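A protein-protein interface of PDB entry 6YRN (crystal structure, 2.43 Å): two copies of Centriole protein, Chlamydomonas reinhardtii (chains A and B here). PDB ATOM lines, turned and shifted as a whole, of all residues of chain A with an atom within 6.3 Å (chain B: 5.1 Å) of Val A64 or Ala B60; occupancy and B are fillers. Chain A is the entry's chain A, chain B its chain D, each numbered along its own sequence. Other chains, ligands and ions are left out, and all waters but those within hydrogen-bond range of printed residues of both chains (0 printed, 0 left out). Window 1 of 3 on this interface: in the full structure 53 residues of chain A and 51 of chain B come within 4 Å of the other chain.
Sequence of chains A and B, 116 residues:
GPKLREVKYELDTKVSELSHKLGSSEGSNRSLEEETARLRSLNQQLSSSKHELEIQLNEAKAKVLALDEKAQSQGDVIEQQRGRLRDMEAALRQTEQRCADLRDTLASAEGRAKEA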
ATOM      1  N   LEU A  57       9.664   1.798 -18.858  1.00  0.00           N
ATOM      2  CA  LEU A  57       9.956   2.911 -17.957  1.00  0.00           C
ATOM      3  C   LEU A  57      11.066   2.562 -16.993  1.00  0.00           C
ATOM      4  O   LEU A  57      12.010   3.350 -16.825  1.00  0.00           O
ATOM      5  CB  LEU A  57       8.705   3.375 -17.199  1.00  0.00           C
ATOM      6  CG  LEU A  57       8.886   4.606 -16.269  1.00  0.00           C
ATOM      7  CD1 LEU A  57       9.297   5.871 -17.078  1.00  0.00           C
ATOM      8  CD2 LEU A  57       7.628   4.856 -15.452  1.00  0.00           C
ATOM      9  N   GLU A  59      13.439   0.405 -17.335  1.00  0.00           N
ATOM     10  CA  GLU A  59      14.673   0.295 -18.117  1.00  0.00           C
ATOM     11  C   GLU A  59      15.223   1.681 -18.420  1.00  0.00           C
ATOM     12  O   GLU A  59      16.428   1.898 -18.283  1.00  0.00           O
ATOM     13  CB  GLU A  59      14.435  -0.466 -19.443  1.00  0.00           C
ATOM     14  CG  GLU A  59      14.253  -1.967 -19.296  1.00  0.00           C
ATOM     15  CD  GLU A  59      13.974  -2.772 -20.554  1.00  0.00           C
ATOM     16  OE1 GLU A  59      13.542  -2.196 -21.583  1.00  0.00           O
ATOM     17  OE2 GLU A  59      14.164  -4.008 -20.486  1.00  0.00           O
ATOM     18  N   ALA A  60      14.335   2.612 -18.852  1.00  0.00           N
ATOM     19  CA  ALA A  60      14.705   3.970 -19.207  1.00  0.00           C
ATOM     20  C   ALA A  60      15.219   4.699 -17.978  1.00  0.00           C
ATOM     21  O   ALA A  60      16.229   5.386 -18.102  1.00  0.00           O
ATOM     22  CB  ALA A  60      13.521   4.699 -19.811  1.00  0.00           C
ATOM     23  N   LYS A  61      14.540   4.539 -16.792  1.00  0.00           N
ATOM     24  CA  LYS A  61      14.951   5.184 -15.541  1.00  0.00           C
ATOM     25  C   LYS A  61      16.337   4.703 -15.102  1.00  0.00           C
ATOM     26  O   LYS A  61      17.163   5.508 -14.657  1.00  0.00           O
ATOM     27  CB  LYS A  61      13.902   4.981 -14.438  1.00  0.00           C
ATOM     28  CG  LYS A  61      12.616   5.781 -14.638  1.00  0.00           C
ATOM     29  CD  LYS A  61      11.811   5.883 -13.341  1.00  0.00           C
ATOM     30  CE  LYS A  61      11.188   7.243 -13.152  1.00  0.00           C
ATOM     31  NZ  LYS A  61      11.786   7.967 -11.986  1.00  0.00           N
ATOM     32  N   ALA A  62      16.604   3.396 -15.287  1.00  0.00           N
ATOM     33  CA  ALA A  62      17.891   2.761 -14.992  1.00  0.00           C
ATOM     34  C   ALA A  62      19.014   3.371 -15.874  1.00  0.00           C
ATOM     35  O   ALA A  62      20.086   3.726 -15.362  1.00  0.00           O
ATOM     36  CB  ALA A  62      17.788   1.264 -15.249  1.00  0.00           C
ATOM     37  N   LYS A  63      18.739   3.502 -17.196  1.00  0.00           N
ATOM     38  CA  LYS A  63      19.654   4.050 -18.193  1.00  0.00           C
ATOM     39  C   LYS A  63      19.950   5.514 -17.894  1.00  0.00           C
ATOM     40  O   LYS A  63      21.105   5.919 -18.021  1.00  0.00           O
ATOM     41  CB  LYS A  63      19.150   3.822 -19.624  1.00  0.00           C
ATOM     42  CG  LYS A  63      20.171   4.178 -20.706  1.00  0.00           C
ATOM     43  CD  LYS A  63      20.484   3.025 -21.683  1.00  0.00           C
ATOM     44  CE  LYS A  63      21.824   3.161 -22.396  1.00  0.00           C
ATOM     45  NZ  LYS A  63      21.746   4.042 -23.590  1.00  0.00           N
ATOM     46  N   VAL A  64      18.958   6.282 -17.401  1.00  0.00           N
ATOM     47  CA  VAL A  64      19.146   7.685 -16.992  1.00  0.00           C
ATOM     48  C   VAL A  64      20.209   7.737 -15.885  1.00  0.00           C
ATOM     49  O   VAL A  64      21.183   8.453 -16.039  1.00  0.00           O
ATOM     50  CB  VAL A  64      17.824   8.378 -16.571  1.00  0.00           C
ATOM     51  CG1 VAL A  64      18.080   9.651 -15.763  1.00  0.00           C
ATOM     52  CG2 VAL A  64      16.956   8.693 -17.780  1.00  0.00           C
ATOM     53  N   LEU A  65      20.062   6.930 -14.813  1.00  0.00           N
ATOM     54  CA  LEU A  65      21.040   6.885 -13.718  1.00  0.00           C
ATOM     55  C   LEU A  65      22.460   6.563 -14.177  1.00  0.00           C
ATOM     56  O   LEU A  65      23.411   7.198 -13.733  1.00  0.00           O
ATOM     57  CB  LEU A  65      20.600   5.919 -12.604  1.00  0.00           C
ATOM     58  CG  LEU A  65      19.309   6.227 -11.831  1.00  0.00           C
ATOM     59  CD1 LEU A  65      19.093   5.190 -10.756  1.00  0.00           C
ATOM     60  CD2 LEU A  65      19.325   7.597 -11.195  1.00  0.00           C
ATOM     61  N   ALA A  66      22.604   5.585 -15.068  1.00  0.00           N
ATOM     62  CA  ALA A  66      23.902   5.175 -15.615  1.00  0.00           C
ATOM     63  C   ALA A  66      24.534   6.300 -16.462  1.00  0.00           C
ATOM     64  O   ALA A  66      25.723   6.572 -16.326  1.00  0.00           O
ATOM     65  CB  ALA A  66      23.738   3.909 -16.443  1.00  0.00           C
ATOM     66  N   LEU A  67      23.725   6.978 -17.283  1.00  0.00           N
ATOM     67  CA  LEU A  67      24.157   8.097 -18.116  1.00  0.00           C
ATOM     68  C   LEU A  67      24.494   9.337 -17.303  1.00  0.00           C
ATOM     69  O   LEU A  67      25.476  10.012 -17.625  1.00  0.00           O
ATOM     70  CB  LEU A  67      23.138   8.423 -19.205  1.00  0.00           C
ATOM     71  CG  LEU A  67      23.029   7.411 -20.333  1.00  0.00           C
ATOM     72  CD1 LEU A  67      21.746   7.627 -21.121  1.00  0.00           C
ATOM     73  CD2 LEU A  67      24.252   7.461 -21.249  1.00  0.00           C
ATOM     74  N   ASP A  68      23.714   9.618 -16.238  1.00  0.00           N
ATOM     75  CA  ASP A  68      23.961  10.737 -15.335  1.00  0.00           C
ATOM     76  C   ASP A  68      25.332  10.525 -14.681  1.00  0.00           C
ATOM     77  O   ASP A  68      26.138  11.446 -14.645  1.00  0.00           O
ATOM     78  CB  ASP A  68      22.883  10.794 -14.227  1.00  0.00           C
ATOM     79  CG  ASP A  68      21.663  11.691 -14.447  1.00  0.00           C
ATOM     80  OD1 ASP A  68      21.695  12.530 -15.381  1.00  0.00           O
ATOM     81  OD2 ASP A  68      20.650  11.528 -13.699  1.00  0.00           O
ATOM     82  N   GLU A  69      25.595   9.290 -14.203  1.00  0.00           N
ATOM     83  CA  GLU A  69      26.834   8.870 -13.561  1.00  0.00           C
ATOM     84  C   GLU A  69      28.022   9.067 -14.510  1.00  0.00           C
ATOM     85  O   GLU A  69      29.030   9.645 -14.099  1.00  0.00           O
ATOM     86  CB  GLU A  69      26.736   7.397 -13.107  1.00  0.00           C
ATOM     87  CG  GLU A  69      27.917   6.953 -12.242  1.00  0.00           C
ATOM     88  CD  GLU A  69      28.072   5.487 -11.882  1.00  0.00           C
ATOM     89  OE1 GLU A  69      29.018   5.191 -11.118  1.00  0.00           O
ATOM     90  OE2 GLU A  69      27.277   4.638 -12.352  1.00  0.00           O
ATOM     91  N   GLN B  56       5.466   9.700 -18.811  1.00  0.00           N
ATOM     92  CA  GLN B  56       6.686   9.427 -18.060  1.00  0.00           C
ATOM     93  C   GLN B  56       7.745   8.787 -18.913  1.00  0.00           C
ATOM     94  O   GLN B  56       8.909   9.169 -18.790  1.00  0.00           O
ATOM     95  CB  GLN B  56       6.399   8.548 -16.841  1.00  0.00           C
ATOM     96  CG  GLN B  56       5.985   9.324 -15.623  1.00  0.00           C
ATOM     97  CD  GLN B  56       5.664   8.388 -14.469  1.00  0.00           C
ATOM     98  OE1 GLN B  56       6.518   7.654 -13.941  1.00  0.00           O
ATOM     99  NE2 GLN B  56       4.422   8.381 -14.068  1.00  0.00           N
ATOM    100  N   LEU B  57       7.356   7.826 -19.760  1.00  0.00           N
ATOM    101  CA  LEU B  57       8.269   7.114 -20.663  1.00  0.00           C
ATOM    102  C   LEU B  57       8.853   8.069 -21.679  1.00  0.00           C
ATOM    103  O   LEU B  57      10.071   8.066 -21.861  1.00  0.00           O
ATOM    104  CB  LEU B  57       7.586   5.936 -21.362  1.00  0.00           C
ATOM    105  CG  LEU B  57       8.455   5.023 -22.219  1.00  0.00           C
ATOM    106  CD1 LEU B  57       9.597   4.405 -21.424  1.00  0.00           C
ATOM    107  CD2 LEU B  57       7.615   3.957 -22.909  1.00  0.00           C
ATOM    108  N   ASN B  58       8.009   8.919 -22.290  1.00  0.00           N
ATOM    109  CA  ASN B  58       8.459   9.912 -23.262  1.00  0.00           C
ATOM    110  C   ASN B  58       9.493  10.841 -22.681  1.00  0.00           C
ATOM    111  O   ASN B  58      10.494  11.103 -23.350  1.00  0.00           O
ATOM    112  CB  ASN B  58       7.281  10.677 -23.880  1.00  0.00           C
ATOM    113  CG  ASN B  58       6.423   9.831 -24.815  1.00  0.00           C
ATOM    114  OD1 ASN B  58       6.754   8.677 -25.178  1.00  0.00           O
ATOM    115  ND2 ASN B  58       5.294  10.392 -25.227  1.00  0.00           N
ATOM    116  N   GLU B  59       9.294  11.276 -21.417  1.00  0.00           N
ATOM    117  CA  GLU B  59      10.209  12.159 -20.692  1.00  0.00           C
ATOM    118  C   GLU B  59      11.533  11.447 -20.411  1.00  0.00           C
ATOM    119  O   GLU B  59      12.593  12.046 -20.596  1.00  0.00           O
ATOM    120  CB  GLU B  59       9.574  12.631 -19.362  1.00  0.00           C
ATOM    121  CG  GLU B  59       8.467  13.668 -19.520  1.00  0.00           C
ATOM    122  CD  GLU B  59       7.718  14.129 -18.278  1.00  0.00           C
ATOM    123  OE1 GLU B  59       7.821  13.459 -17.220  1.00  0.00           O
ATOM    124  OE2 GLU B  59       6.999  15.154 -18.380  1.00  0.00           O
ATOM    125  N   ALA B  60      11.464  10.185 -19.942  1.00  0.00           N
ATOM    126  CA  ALA B  60      12.624   9.362 -19.609  1.00  0.00           C
ATOM    127  C   ALA B  60      13.414   9.064 -20.861  1.00  0.00           C
ATOM    128  O   ALA B  60      14.624   9.195 -20.830  1.00  0.00           O
ATOM    129  CB  ALA B  60      12.183   8.051 -18.959  1.00  0.00           C
ATOM    130  N   LYS B  61      12.741   8.673 -21.966  1.00  0.00           N
ATOM    131  CA  LYS B  61      13.373   8.377 -23.255  1.00  0.00           C
ATOM    132  C   LYS B  61      14.094   9.599 -23.782  1.00  0.00           C
ATOM    133  O   LYS B  61      15.198   9.454 -24.291  1.00  0.00           O
ATOM    134  CB  LYS B  61      12.368   7.863 -24.308  1.00  0.00           C
ATOM    135  CG  LYS B  61      11.932   6.425 -24.072  1.00  0.00           C
ATOM    136  CD  LYS B  61      11.352   5.743 -25.341  1.00  0.00           C
ATOM    137  CE  LYS B  61       9.869   5.980 -25.596  1.00  0.00           C
ATOM    138  NZ  LYS B  61       9.413   5.317 -26.832  1.00  0.00           N
ATOM    139  N   ALA B  62      13.499  10.799 -23.621  1.00  0.00           N
ATOM    140  CA  ALA B  62      14.073  12.085 -24.037  1.00  0.00           C
ATOM    141  C   ALA B  62      15.371  12.343 -23.296  1.00  0.00           C
ATOM    142  O   ALA B  62      16.384  12.651 -23.934  1.00  0.00           O
ATOM    143  CB  ALA B  62      13.093  13.218 -23.778  1.00  0.00           C
ATOM    144  N   LYS B  63      15.344  12.168 -21.957  1.00  0.00           N
ATOM    145  CA  LYS B  63      16.496  12.352 -21.075  1.00  0.00           C
ATOM    146  C   LYS B  63      17.633  11.401 -21.448  1.00  0.00           C
ATOM    147  O   LYS B  63      18.774  11.847 -21.530  1.00  0.00           O
ATOM    148  CB  LYS B  63      16.079  12.254 -19.590  1.00  0.00           C
ATOM    149  CG  LYS B  63      17.208  12.645 -18.640  1.00  0.00           C
ATOM    150  CD  LYS B  63      16.724  13.167 -17.308  1.00  0.00           C
ATOM    151  CE  LYS B  63      17.893  13.445 -16.376  1.00  0.00           C
ATOM    152  NZ  LYS B  63      18.531  14.775 -16.601  1.00  0.00           N
ATOM    153  N   VAL B  64      17.315  10.124 -21.767  1.00  0.00           N
ATOM    154  CA  VAL B  64      18.309   9.131 -22.213  1.00  0.00           C
ATOM    155  C   VAL B  64      19.031   9.642 -23.458  1.00  0.00           C
ATOM    156  O   VAL B  64      20.253   9.732 -23.438  1.00  0.00           O
ATOM    157  CB  VAL B  64      17.678   7.722 -22.442  1.00  0.00           C
ATOM    158  CG1 VAL B  64      18.578   6.810 -23.271  1.00  0.00           C
ATOM    159  CG2 VAL B  64      17.288   7.054 -21.129  1.00  0.00           C
ATOM    160  N   LEU B  67      21.358  12.619 -22.725  1.00  0.00           N
ATOM    161  CA  LEU B  67      22.521  12.168 -21.975  1.00  0.00           C
ATOM    162  C   LEU B  67      23.490  11.376 -22.825  1.00  0.00           C
ATOM    163  O   LEU B  67      24.696  11.581 -22.695  1.00  0.00           O
ATOM    164  CB  LEU B  67      22.110  11.406 -20.725  1.00  0.00           C
ATOM    165  CG  LEU B  67      21.448  12.218 -19.594  1.00  0.00           C
ATOM    166  CD1 LEU B  67      20.781  11.276 -18.579  1.00  0.00           C
ATOM    167  CD2 LEU B  67      22.428  13.107 -18.906  1.00  0.00           C
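Among the printed residues, pairs that only touch across the chains: Leu A57 with Gln B56, Leu A57 with Leu B57, Ala A60 with Ala B60, Ala A60 with Val B64, Val A64 with Ala B60, Val A64 with Lys B63, Val A64 with Val B64, Val A64 with Leu B67, Leu A67 with Val B64, Leu A67 with Leu B67 and Asp A68 with Leu B67.
Printed residues of chain B within 4 Å of Leu A57: Gln B56 (3.4 Å) and Leu B57 (3.7 Å).
Val A64 touches just these residues of chain B: Ala B60 (3.9 Å), Lys B63 (3.8 Å), Val B64 (3.7 Å) and Leu B67 (3.8 Å).
Glu A69 touches none of the printed residues of chain B.
Of the printed residues of chain A, Gln B56 touches Leu A57.
Of chain A, only Ala A60 and Val A64 come within 4 Å of Ala B60.
Lys B61 touches none of the printed residues of chain A.
The nearest printed residue of chain B that does not touch Val A64 is Lys B61 (5.9 Å).
Leu B57 touches its own counterpart, Leu A57.
Ala A60 touches its own counterpart, Ala B60.
Ala A60 touches Val B64, and with the chains exchanged Val A64 touches Ala B60.
Val A64 touches Lys B63, but with the chains exchanged Lys A63 does not touch Val B64 (4.01 Å).
Of the 10 printed residues of chain B, 6 touch a printed residue of chain A.
Among the printed residues, no Asp or Glu carboxylate lies within 4 Å of a Lys or Arg side-chain nitrogen of the other chain.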
